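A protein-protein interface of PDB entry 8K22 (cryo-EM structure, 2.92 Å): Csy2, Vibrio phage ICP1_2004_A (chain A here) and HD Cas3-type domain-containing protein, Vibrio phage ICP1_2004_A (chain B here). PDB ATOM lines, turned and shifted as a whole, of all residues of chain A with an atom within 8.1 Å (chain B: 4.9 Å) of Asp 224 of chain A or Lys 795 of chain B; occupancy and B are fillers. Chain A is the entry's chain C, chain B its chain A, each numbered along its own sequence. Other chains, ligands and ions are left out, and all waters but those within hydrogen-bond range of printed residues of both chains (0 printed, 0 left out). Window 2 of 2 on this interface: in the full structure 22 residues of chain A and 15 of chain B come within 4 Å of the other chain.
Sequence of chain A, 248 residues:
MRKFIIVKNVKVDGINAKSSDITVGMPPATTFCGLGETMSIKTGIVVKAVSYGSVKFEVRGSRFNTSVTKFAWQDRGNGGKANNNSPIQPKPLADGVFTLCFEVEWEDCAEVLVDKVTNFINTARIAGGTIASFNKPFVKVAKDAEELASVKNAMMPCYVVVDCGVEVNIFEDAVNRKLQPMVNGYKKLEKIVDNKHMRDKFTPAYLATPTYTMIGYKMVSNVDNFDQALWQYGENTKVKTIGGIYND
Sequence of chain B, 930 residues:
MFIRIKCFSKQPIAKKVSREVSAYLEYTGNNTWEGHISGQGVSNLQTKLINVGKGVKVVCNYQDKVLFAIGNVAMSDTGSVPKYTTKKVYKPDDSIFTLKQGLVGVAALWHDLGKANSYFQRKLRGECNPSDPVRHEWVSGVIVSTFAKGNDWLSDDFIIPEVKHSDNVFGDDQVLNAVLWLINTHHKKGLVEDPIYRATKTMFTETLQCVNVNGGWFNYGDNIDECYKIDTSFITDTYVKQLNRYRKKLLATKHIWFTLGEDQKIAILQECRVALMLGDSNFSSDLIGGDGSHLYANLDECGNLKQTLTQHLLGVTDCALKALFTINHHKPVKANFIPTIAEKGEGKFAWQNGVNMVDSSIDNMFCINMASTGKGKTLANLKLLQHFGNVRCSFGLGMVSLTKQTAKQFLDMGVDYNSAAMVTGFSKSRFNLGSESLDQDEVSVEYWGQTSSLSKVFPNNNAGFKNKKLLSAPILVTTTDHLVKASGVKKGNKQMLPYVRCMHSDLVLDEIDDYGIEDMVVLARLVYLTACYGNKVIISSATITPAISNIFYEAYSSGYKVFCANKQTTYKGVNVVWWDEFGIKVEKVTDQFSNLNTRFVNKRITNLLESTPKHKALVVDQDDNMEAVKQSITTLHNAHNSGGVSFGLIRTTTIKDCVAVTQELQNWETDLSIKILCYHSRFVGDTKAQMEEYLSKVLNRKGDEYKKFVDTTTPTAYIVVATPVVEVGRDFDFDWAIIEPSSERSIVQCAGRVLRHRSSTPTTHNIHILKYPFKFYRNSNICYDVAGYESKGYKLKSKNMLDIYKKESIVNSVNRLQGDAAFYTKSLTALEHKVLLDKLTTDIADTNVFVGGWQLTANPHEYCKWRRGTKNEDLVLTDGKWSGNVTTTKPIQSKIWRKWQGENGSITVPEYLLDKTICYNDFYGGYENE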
ATOM      1  N   ALA A 145      15.274  12.906   0.131  1.00  0.00           N
ATOM      2  CA  ALA A 145      15.143  14.355   0.018  1.00  0.00           C
ATOM      3  C   ALA A 145      14.937  14.778  -1.423  1.00  0.00           C
ATOM      4  O   ALA A 145      14.298  15.793  -1.684  1.00  0.00           O
ATOM      5  CB  ALA A 145      16.347  15.058   0.620  1.00  0.00           C
ATOM      6  N   LEU A 148      11.494  14.279  -1.847  1.00  0.00           N
ATOM      7  CA  LEU A 148      10.752  15.328  -1.158  1.00  0.00           C
ATOM      8  C   LEU A 148      10.633  16.507  -2.094  1.00  0.00           C
ATOM      9  O   LEU A 148       9.593  17.157  -2.156  1.00  0.00           O
ATOM     10  CB  LEU A 148      11.475  15.731   0.129  1.00  0.00           C
ATOM     11  CG  LEU A 148      10.881  16.824   1.011  1.00  0.00           C
ATOM     12  CD1 LEU A 148       9.626  16.323   1.701  1.00  0.00           C
ATOM     13  CD2 LEU A 148      11.899  17.317   2.026  1.00  0.00           C
ATOM     14  N   ALA A 149      11.694  16.770  -2.847  1.00  0.00           N
ATOM     15  CA  ALA A 149      11.663  17.858  -3.807  1.00  0.00           C
ATOM     16  C   ALA A 149      10.800  17.519  -5.004  1.00  0.00           C
ATOM     17  O   ALA A 149      10.312  18.413  -5.684  1.00  0.00           O
ATOM     18  CB  ALA A 149      13.062  18.203  -4.251  1.00  0.00           C
ATOM     19  N   LYS A 152       7.560  18.483  -3.781  1.00  0.00           N
ATOM     20  CA  LYS A 152       7.571  19.937  -3.751  1.00  0.00           C
ATOM     21  C   LYS A 152       7.276  20.521  -5.126  1.00  0.00           C
ATOM     22  O   LYS A 152       6.397  21.371  -5.268  1.00  0.00           O
ATOM     23  CB  LYS A 152       8.943  20.392  -3.266  1.00  0.00           C
ATOM     24  CG  LYS A 152       9.143  21.881  -3.141  1.00  0.00           C
ATOM     25  CD  LYS A 152      10.510  22.174  -2.554  1.00  0.00           C
ATOM     26  CE  LYS A 152      11.611  21.718  -3.492  1.00  0.00           C
ATOM     27  NZ  LYS A 152      11.888  22.720  -4.557  1.00  0.00           N
ATOM     28  N   ASN A 153       7.990  20.057  -6.145  1.00  0.00           N
ATOM     29  CA  ASN A 153       7.809  20.601  -7.488  1.00  0.00           C
ATOM     30  C   ASN A 153       6.535  20.109  -8.161  1.00  0.00           C
ATOM     31  O   ASN A 153       6.189  20.580  -9.239  1.00  0.00           O
ATOM     32  CB  ASN A 153       9.030  20.302  -8.357  1.00  0.00           C
ATOM     33  CG  ASN A 153      10.242  21.117  -7.950  1.00  0.00           C
ATOM     34  OD1 ASN A 153      10.252  21.747  -6.895  1.00  0.00           O
ATOM     35  ND2 ASN A 153      11.270  21.108  -8.787  1.00  0.00           N
ATOM     36  N   VAL A 162       6.342  30.555   3.598  1.00  0.00           N
ATOM     37  CA  VAL A 162       7.508  30.219   4.403  1.00  0.00           C
ATOM     38  C   VAL A 162       7.609  31.202   5.563  1.00  0.00           C
ATOM     39  O   VAL A 162       7.342  32.402   5.425  1.00  0.00           O
ATOM     40  CB  VAL A 162       8.808  30.178   3.566  1.00  0.00           C
ATOM     41  CG1 VAL A 162       8.747  29.037   2.568  1.00  0.00           C
ATOM     42  CG2 VAL A 162       9.047  31.484   2.830  1.00  0.00           C
ATOM     43  N   LYS A 218       7.178  32.468  -1.526  1.00  0.00           N
ATOM     44  CA  LYS A 218       8.190  32.047  -2.493  1.00  0.00           C
ATOM     45  C   LYS A 218       7.529  30.960  -3.337  1.00  0.00           C
ATOM     46  O   LYS A 218       6.715  30.202  -2.819  1.00  0.00           O
ATOM     47  CB  LYS A 218       9.402  31.480  -1.770  1.00  0.00           C
ATOM     48  CG  LYS A 218      10.636  32.352  -1.864  1.00  0.00           C
ATOM     49  CD  LYS A 218      11.798  31.563  -2.429  1.00  0.00           C
ATOM     50  CE  LYS A 218      12.951  32.480  -2.794  1.00  0.00           C
ATOM     51  NZ  LYS A 218      12.493  33.891  -2.917  1.00  0.00           N
ATOM     52  N   MET A 219       7.849  30.875  -4.627  1.00  0.00           N
ATOM     53  CA  MET A 219       7.308  29.801  -5.467  1.00  0.00           C
ATOM     54  C   MET A 219       7.815  28.489  -4.935  1.00  0.00           C
ATOM     55  O   MET A 219       8.963  28.394  -4.513  1.00  0.00           O
ATOM     56  CB  MET A 219       7.749  29.915  -6.924  1.00  0.00           C
ATOM     57  CG  MET A 219       6.831  30.723  -7.818  1.00  0.00           C
ATOM     58  SD  MET A 219       5.330  29.901  -8.373  1.00  0.00           S
ATOM     59  CE  MET A 219       5.112  30.669  -9.975  1.00  0.00           C
ATOM     60  N   VAL A 220       6.982  27.466  -4.985  1.00  0.00           N
ATOM     61  CA  VAL A 220       7.371  26.188  -4.413  1.00  0.00           C
ATOM     62  C   VAL A 220       8.687  25.598  -4.983  1.00  0.00           C
ATOM     63  O   VAL A 220       9.437  24.971  -4.241  1.00  0.00           O
ATOM     64  CB  VAL A 220       6.175  25.202  -4.393  1.00  0.00           C
ATOM     65  CG1 VAL A 220       5.911  24.581  -5.747  1.00  0.00           C
ATOM     66  CG2 VAL A 220       6.318  24.168  -3.292  1.00  0.00           C
ATOM     67  N   SER A 221       9.013  25.843  -6.253  1.00  0.00           N
ATOM     68  CA  SER A 221      10.276  25.320  -6.775  1.00  0.00           C
ATOM     69  C   SER A 221      11.469  26.098  -6.240  1.00  0.00           C
ATOM     70  O   SER A 221      12.549  25.527  -6.062  1.00  0.00           O
ATOM     71  CB  SER A 221      10.302  25.355  -8.299  1.00  0.00           C
ATOM     72  OG  SER A 221      10.822  26.588  -8.759  1.00  0.00           O
ATOM     73  N   ASN A 222      11.296  27.390  -5.981  1.00  0.00           N
ATOM     74  CA  ASN A 222      12.378  28.202  -5.449  1.00  0.00           C
ATOM     75  C   ASN A 222      12.590  27.997  -3.958  1.00  0.00           C
ATOM     76  O   ASN A 222      13.568  28.513  -3.411  1.00  0.00           O
ATOM     77  CB  ASN A 222      12.114  29.676  -5.738  1.00  0.00           C
ATOM     78  CG  ASN A 222      12.107  29.978  -7.215  1.00  0.00           C
ATOM     79  OD1 ASN A 222      12.960  29.498  -7.960  1.00  0.00           O
ATOM     80  ND2 ASN A 222      11.139  30.770  -7.654  1.00  0.00           N
ATOM     81  N   VAL A 223      11.700  27.263  -3.291  1.00  0.00           N
ATOM     82  CA  VAL A 223      11.919  26.907  -1.898  1.00  0.00           C
ATOM     83  C   VAL A 223      12.912  25.755  -1.839  1.00  0.00           C
ATOM     84  O   VAL A 223      12.721  24.719  -2.487  1.00  0.00           O
ATOM     85  CB  VAL A 223      10.589  26.537  -1.227  1.00  0.00           C
ATOM     86  CG1 VAL A 223      10.803  26.219   0.228  1.00  0.00           C
ATOM     87  CG2 VAL A 223       9.602  27.664  -1.377  1.00  0.00           C
ATOM     88  N   ASP A 224      13.992  25.942  -1.079  1.00  0.00           N
ATOM     89  CA  ASP A 224      15.054  24.940  -1.028  1.00  0.00           C
ATOM     90  C   ASP A 224      14.613  23.697  -0.265  1.00  0.00           C
ATOM     91  O   ASP A 224      14.795  22.568  -0.731  1.00  0.00           O
ATOM     92  CB  ASP A 224      16.312  25.547  -0.404  1.00  0.00           C
ATOM     93  CG  ASP A 224      16.008  26.439   0.789  1.00  0.00           C
ATOM     94  OD1 ASP A 224      14.889  26.351   1.338  1.00  0.00           O
ATOM     95  OD2 ASP A 224      16.890  27.233   1.177  1.00  0.00           O
ATOM     96  N   ASN A 225      14.024  23.886   0.910  1.00  0.00           N
ATOM     97  CA  ASN A 225      13.594  22.789   1.764  1.00  0.00           C
ATOM     98  C   ASN A 225      12.077  22.806   1.858  1.00  0.00           C
ATOM     99  O   ASN A 225      11.494  23.795   2.311  1.00  0.00           O
ATOM    100  CB  ASN A 225      14.221  22.902   3.152  1.00  0.00           C
ATOM    101  CG  ASN A 225      14.065  21.637   3.967  1.00  0.00           C
ATOM    102  OD1 ASN A 225      13.659  20.597   3.449  1.00  0.00           O
ATOM    103  ND2 ASN A 225      14.389  21.718   5.251  1.00  0.00           N
ATOM    104  N   PHE A 226      11.447  21.696   1.466  1.00  0.00           N
ATOM    105  CA  PHE A 226       9.992  21.593   1.505  1.00  0.00           C
ATOM    106  C   PHE A 226       9.446  21.578   2.927  1.00  0.00           C
ATOM    107  O   PHE A 226       8.269  21.893   3.127  1.00  0.00           O
ATOM    108  CB  PHE A 226       9.547  20.339   0.753  1.00  0.00           C
ATOM    109  CG  PHE A 226       8.078  20.291   0.470  1.00  0.00           C
ATOM    110  CD1 PHE A 226       7.392  21.433   0.093  1.00  0.00           C
ATOM    111  CD2 PHE A 226       7.382  19.099   0.576  1.00  0.00           C
ATOM    112  CE1 PHE A 226       6.040  21.388  -0.165  1.00  0.00           C
ATOM    113  CE2 PHE A 226       6.028  19.047   0.320  1.00  0.00           C
ATOM    114  CZ  PHE A 226       5.359  20.191  -0.051  1.00  0.00           C
ATOM    115  N   ASP A 227      10.275  21.244   3.918  1.00  0.00           N
ATOM    116  CA  ASP A 227       9.853  21.308   5.311  1.00  0.00           C
ATOM    117  C   ASP A 227       9.618  22.734   5.788  1.00  0.00           C
ATOM    118  O   ASP A 227       8.919  22.931   6.787  1.00  0.00           O
ATOM    119  CB  ASP A 227      10.892  20.631   6.204  1.00  0.00           C
ATOM    120  CG  ASP A 227      10.823  19.124   6.128  1.00  0.00           C
ATOM    121  OD1 ASP A 227       9.943  18.613   5.407  1.00  0.00           O
ATOM    122  OD2 ASP A 227      11.646  18.451   6.783  1.00  0.00           O
ATOM    123  N   GLN A 228      10.183  23.731   5.106  1.00  0.00           N
ATOM    124  CA  GLN A 228       9.939  25.124   5.448  1.00  0.00           C
ATOM    125  C   GLN A 228       8.640  25.656   4.862  1.00  0.00           C
ATOM    126  O   GLN A 228       8.303  26.820   5.103  1.00  0.00           O
ATOM    127  CB  GLN A 228      11.109  25.992   4.982  1.00  0.00           C
ATOM    128  CG  GLN A 228      12.196  26.160   6.025  1.00  0.00           C
ATOM    129  CD  GLN A 228      13.579  26.227   5.416  1.00  0.00           C
ATOM    130  OE1 GLN A 228      13.739  26.136   4.200  1.00  0.00           O
ATOM    131  NE2 GLN A 228      14.589  26.382   6.262  1.00  0.00           N
ATOM    132  N   ALA A 229       7.916  24.845   4.092  1.00  0.00           N
ATOM    133  CA  ALA A 229       6.609  25.215   3.575  1.00  0.00           C
ATOM    134  C   ALA A 229       5.478  24.375   4.143  1.00  0.00           C
ATOM    135  O   ALA A 229       4.310  24.704   3.910  1.00  0.00           O
ATOM    136  CB  ALA A 229       6.592  25.111   2.044  1.00  0.00           C
ATOM    137  N   ILE A 245      12.396  28.532  10.592  1.00  0.00           N
ATOM    138  CA  ILE A 245      12.439  29.852   9.975  1.00  0.00           C
ATOM    139  C   ILE A 245      13.142  29.755   8.628  1.00  0.00           C
ATOM    140  O   ILE A 245      14.233  29.184   8.523  1.00  0.00           O
ATOM    141  CB  ILE A 245      13.150  30.853  10.899  1.00  0.00           C
ATOM    142  CG1 ILE A 245      12.457  30.898  12.260  1.00  0.00           C
ATOM    143  CG2 ILE A 245      13.191  32.232  10.275  1.00  0.00           C
ATOM    144  CD1 ILE A 245      11.010  31.310  12.191  1.00  0.00           C
ATOM    145  N   TYR A 246      12.508  30.300   7.592  1.00  0.00           N
ATOM    146  CA  TYR A 246      13.136  30.366   6.280  1.00  0.00           C
ATOM    147  C   TYR A 246      14.268  31.384   6.299  1.00  0.00           C
ATOM    148  O   TYR A 246      14.100  32.506   6.783  1.00  0.00           O
ATOM    149  CB  TYR A 246      12.103  30.737   5.219  1.00  0.00           C
ATOM    150  CG  TYR A 246      12.552  30.500   3.798  1.00  0.00           C
ATOM    151  CD1 TYR A 246      12.384  29.260   3.198  1.00  0.00           C
ATOM    152  CD2 TYR A 246      13.143  31.515   3.058  1.00  0.00           C
ATOM    153  CE1 TYR A 246      12.792  29.036   1.901  1.00  0.00           C
ATOM    154  CE2 TYR A 246      13.555  31.300   1.760  1.00  0.00           C
ATOM    155  CZ  TYR A 246      13.375  30.059   1.187  1.00  0.00           C
ATOM    156  OH  TYR A 246      13.783  29.832  -0.106  1.00  0.00           O
ATOM    157  N   ASN A 247      15.420  30.992   5.768  1.00  0.00           N
ATOM    158  CA  ASN A 247      16.589  31.862   5.757  1.00  0.00           C
ATOM    159  C   ASN A 247      16.885  32.363   4.349  1.00  0.00           C
ATOM    160  O   ASN A 247      16.892  31.586   3.394  1.00  0.00           O
ATOM    161  CB  ASN A 247      17.806  31.127   6.320  1.00  0.00           C
ATOM    162  CG  ASN A 247      17.752  30.983   7.826  1.00  0.00           C
ATOM    163  OD1 ASN A 247      17.084  31.758   8.511  1.00  0.00           O
ATOM    164  ND2 ASN A 247      18.456  29.987   8.351  1.00  0.00           N
ATOM    165  N   ASN B 781      20.101  28.717  -9.653  1.00  0.00           N
ATOM    166  CA  ASN B 781      19.446  27.935  -8.611  1.00  0.00           C
ATOM    167  C   ASN B 781      20.204  26.623  -8.425  1.00  0.00           C
ATOM    168  O   ASN B 781      20.506  26.222  -7.296  1.00  0.00           O
ATOM    169  CB  ASN B 781      17.950  27.786  -9.009  1.00  0.00           C
ATOM    170  CG  ASN B 781      17.120  26.663  -8.276  1.00  0.00           C
ATOM    171  OD1 ASN B 781      17.588  25.674  -7.715  1.00  0.00           O
ATOM    172  ND2 ASN B 781      15.810  26.874  -8.317  1.00  0.00           N
ATOM    173  N   ILE B 782      20.530  25.948  -9.526  1.00  0.00           N
ATOM    174  CA  ILE B 782      21.240  24.672  -9.503  1.00  0.00           C
ATOM    175  C   ILE B 782      22.238  24.669 -10.653  1.00  0.00           C
ATOM    176  O   ILE B 782      21.860  24.909 -11.805  1.00  0.00           O
ATOM    177  CB  ILE B 782      20.263  23.483  -9.619  1.00  0.00           C
ATOM    178  CG1 ILE B 782      19.639  23.161  -8.267  1.00  0.00           C
ATOM    179  CG2 ILE B 782      20.957  22.244 -10.104  1.00  0.00           C
ATOM    180  CD1 ILE B 782      18.534  22.144  -8.346  1.00  0.00           C
ATOM    181  N   GLU B 790      24.893  17.212  -6.891  1.00  0.00           N
ATOM    182  CA  GLU B 790      23.882  18.206  -6.571  1.00  0.00           C
ATOM    183  C   GLU B 790      22.607  17.888  -7.337  1.00  0.00           C
ATOM    184  O   GLU B 790      22.644  17.299  -8.419  1.00  0.00           O
ATOM    185  CB  GLU B 790      24.364  19.608  -6.920  1.00  0.00           C
ATOM    186  CG  GLU B 790      23.860  20.674  -5.971  1.00  0.00           C
ATOM    187  CD  GLU B 790      23.964  22.073  -6.539  1.00  0.00           C
ATOM    188  OE1 GLU B 790      23.853  22.229  -7.772  1.00  0.00           O
ATOM    189  OE2 GLU B 790      24.162  23.017  -5.747  1.00  0.00           O
ATOM    190  N   SER B 791      21.472  18.263  -6.760  1.00  0.00           N
ATOM    191  CA  SER B 791      20.181  17.952  -7.361  1.00  0.00           C
ATOM    192  C   SER B 791      19.127  18.872  -6.759  1.00  0.00           C
ATOM    193  O   SER B 791      19.445  19.818  -6.030  1.00  0.00           O
ATOM    194  CB  SER B 791      19.816  16.484  -7.146  1.00  0.00           C
ATOM    195  OG  SER B 791      19.553  16.227  -5.780  1.00  0.00           O
ATOM    196  N   LYS B 792      17.862  18.580  -7.060  1.00  0.00           N
ATOM    197  CA  LYS B 792      16.763  19.390  -6.551  1.00  0.00           C
ATOM    198  C   LYS B 792      16.481  19.128  -5.081  1.00  0.00           C
ATOM    199  O   LYS B 792      15.950  20.009  -4.401  1.00  0.00           O
ATOM    200  CB  LYS B 792      15.506  19.149  -7.387  1.00  0.00           C
ATOM    201  CG  LYS B 792      15.039  17.707  -7.438  1.00  0.00           C
ATOM    202  CD  LYS B 792      14.521  17.343  -8.818  1.00  0.00           C
ATOM    203  CE  LYS B 792      13.190  18.022  -9.095  1.00  0.00           C
ATOM    204  NZ  LYS B 792      12.165  17.633  -8.091  1.00  0.00           N
ATOM    205  N   GLY B 793      16.824  17.953  -4.575  1.00  0.00           N
ATOM    206  CA  GLY B 793      16.624  17.663  -3.172  1.00  0.00           C
ATOM    207  C   GLY B 793      17.812  18.018  -2.309  1.00  0.00           C
ATOM    208  O   GLY B 793      17.691  18.131  -1.087  1.00  0.00           O
ATOM    209  N   TYR B 794      18.968  18.206  -2.939  1.00  0.00           N
ATOM    210  CA  TYR B 794      20.219  18.495  -2.241  1.00  0.00           C
ATOM    211  C   TYR B 794      20.825  19.718  -2.915  1.00  0.00           C
ATOM    212  O   TYR B 794      21.598  19.593  -3.865  1.00  0.00           O
ATOM    213  CB  TYR B 794      21.163  17.299  -2.280  1.00  0.00           C
ATOM    214  CG  TYR B 794      20.529  16.003  -1.837  1.00  0.00           C
ATOM    215  CD1 TYR B 794      20.504  15.643  -0.496  1.00  0.00           C
ATOM    216  CD2 TYR B 794      19.963  15.134  -2.761  1.00  0.00           C
ATOM    217  CE1 TYR B 794      19.930  14.456  -0.090  1.00  0.00           C
ATOM    218  CE2 TYR B 794      19.383  13.953  -2.366  1.00  0.00           C
ATOM    219  CZ  TYR B 794      19.368  13.619  -1.031  1.00  0.00           C
ATOM    220  OH  TYR B 794      18.790  12.439  -0.640  1.00  0.00           O
ATOM    221  N   LYS B 795      20.473  20.898  -2.417  1.00  0.00           N
ATOM    222  CA  LYS B 795      20.898  22.160  -2.999  1.00  0.00           C
ATOM    223  C   LYS B 795      21.951  22.804  -2.113  1.00  0.00           C
ATOM    224  O   LYS B 795      21.770  22.900  -0.895  1.00  0.00           O
ATOM    225  CB  LYS B 795      19.710  23.107  -3.172  1.00  0.00           C
ATOM    226  CG  LYS B 795      19.323  23.345  -4.610  1.00  0.00           C
ATOM    227  CD  LYS B 795      18.088  24.219  -4.721  1.00  0.00           C
ATOM    228  CE  LYS B 795      16.902  23.585  -4.015  1.00  0.00           C
ATOM    229  NZ  LYS B 795      15.610  24.184  -4.451  1.00  0.00           N
ATOM    230  N   LEU B 796      23.051  23.233  -2.724  1.00  0.00           N
ATOM    231  CA  LEU B 796      24.039  24.015  -2.002  1.00  0.00           C
ATOM    232  C   LEU B 796      23.484  25.400  -1.696  1.00  0.00           C
ATOM    233  O   LEU B 796      22.826  26.019  -2.537  1.00  0.00           O
ATOM    234  CB  LEU B 796      25.326  24.129  -2.812  1.00  0.00           C
ATOM    235  CG  LEU B 796      26.178  22.864  -2.856  1.00  0.00           C
ATOM    236  CD1 LEU B 796      27.075  22.871  -4.077  1.00  0.00           C
ATOM    237  CD2 LEU B 796      26.999  22.735  -1.587  1.00  0.00           C
ATOM    238  N   LYS B 797      23.730  25.870  -0.470  1.00  0.00           N
ATOM    239  CA  LYS B 797      23.279  27.202  -0.080  1.00  0.00           C
ATOM    240  C   LYS B 797      24.022  28.280  -0.858  1.00  0.00           C
ATOM    241  O   LYS B 797      23.422  29.268  -1.294  1.00  0.00           O
ATOM    242  CB  LYS B 797      23.460  27.391   1.426  1.00  0.00           C
ATOM    243  CG  LYS B 797      23.103  28.776   1.943  1.00  0.00           C
ATOM    244  CD  LYS B 797      21.736  28.776   2.610  1.00  0.00           C
ATOM    245  CE  LYS B 797      21.355  30.165   3.096  1.00  0.00           C
ATOM    246  NZ  LYS B 797      19.948  30.222   3.579  1.00  0.00           N
ATOM    247  N   THR B 825      25.247  21.635   2.870  1.00  0.00           N
ATOM    248  CA  THR B 825      24.693  22.714   2.064  1.00  0.00           C
ATOM    249  C   THR B 825      25.712  23.794   1.734  1.00  0.00           C
ATOM    250  O   THR B 825      25.400  24.692   0.947  1.00  0.00           O
ATOM    251  CB  THR B 825      23.496  23.345   2.777  1.00  0.00           C
ATOM    252  OG1 THR B 825      23.893  23.787   4.080  1.00  0.00           O
ATOM    253  CG2 THR B 825      22.370  22.337   2.911  1.00  0.00           C
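Asp 224 of chain A touches just one residue of chain B: Lys 795.
Printed residues of chain A within 4 Å of Lys 795 of chain B: Ser 221 (3.7 Å), Val 223 (3.5 Å) and Asp 224 (3.5 Å).
Printed residues of chain A within 4 Å of Lys 797 of chain B: Asn 247.
Of the printed residues of chain B, Asn 247 of chain A touches Lys 797.
Printed residues of chain B within 4 Å of Asn 222 of chain A: Asn 781.
Of the printed residues of chain A, Tyr 794 of chain B touches Ala 145 (3.6 Å).
Printed residues of chain A within 4 Å of Asn 781 of chain B: Asn 222 (3.9 Å).
Asp 227 of chain A touches none of the printed residues of chain B.
The nearest residue of chain B that does not touch Asp 224 of chain A is Lys 792 of chain B (4.6 Å).
The nearest printed residue of chain A that does not touch Lys 795 of chain B is Lys 152 of chain A (4.001 Å).
The backbone carbonyl oxygen (O) of Ala 149 of chain A is in hydrogen-bond range of the side-chain amino group (NZ) of Lys 792 of chain B, 3.1 Å away.
O of Asn 247 of chain A lies within hydrogen-bond range of NZ of Lys 797 of chain B.
Gly 793 of chain B touches Ala 145 of chain A (CA to O, 3.3 Å).
Tyr 794 of chain B touches Ala 145 of chain A (OH to N, 3.6 Å).
Gly 793 of chain B touches Ala 149 of chain A.
Asn 153 of chain A touches Lys 792 of chain B.
Lys 795 of chain B touches Ser 221 of chain A (NZ to O, 3.7 Å).
OD1 of Asn 222 of chain A touches ND2 of Asn 781 of chain B, at 3.9 Å.
Val 223 of chain A touches Lys 795 of chain B (O to NZ, 3.5 Å).
Lys 795 of chain B touches Asp 224 of chain A.
Printed residues of chain B that touch a printed residue of chain A: Asn 781, Lys 792, Gly 793, Tyr 794, Lys 795 and Lys 797.
Hydrophobic or aromatic side chains of chain B within 4 Å of the printed part of chain A: Tyr 794.
Of the 21 printed residues of chain A, 8 touch a printed residue of chain B.
Among the printed residues, no Asp or Glu carboxylate lies within 4 Å of a Lys or Arg side-chain nitrogen of the other chain.
The side-chain amide oxygen (OD1) of Asn 153 of chain A lies within hydrogen-bond range of the side-chain amino group (NZ) of Lys 152 of chain A (3.0 Å).
The backbone carbonyl oxygen of Ser 221 of chain A lies within hydrogen-bond range of the side-chain amino group of Lys 152 of chain A, 3.3 Å away.
The backbone carbonyl oxygen of Val 223 of chain A sits at hydrogen-bond distance from the side-chain amino group of Lys 152 of chain A.
The side-chain carboxylate of Asp 224 of chain A sits close to the side-chain amide oxygen of Gln 228 of chain A, 3.1 Å away.
The side-chain hydroxyl of Ser 791 of chain B lies close to the backbone NH of Gly 793 of chain B (3.4 Å).
The backbone carbonyl oxygen of Thr 825 of chain B sits at hydrogen-bond distance from the backbone NH of Lys 797 of chain B (2.5 Å).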
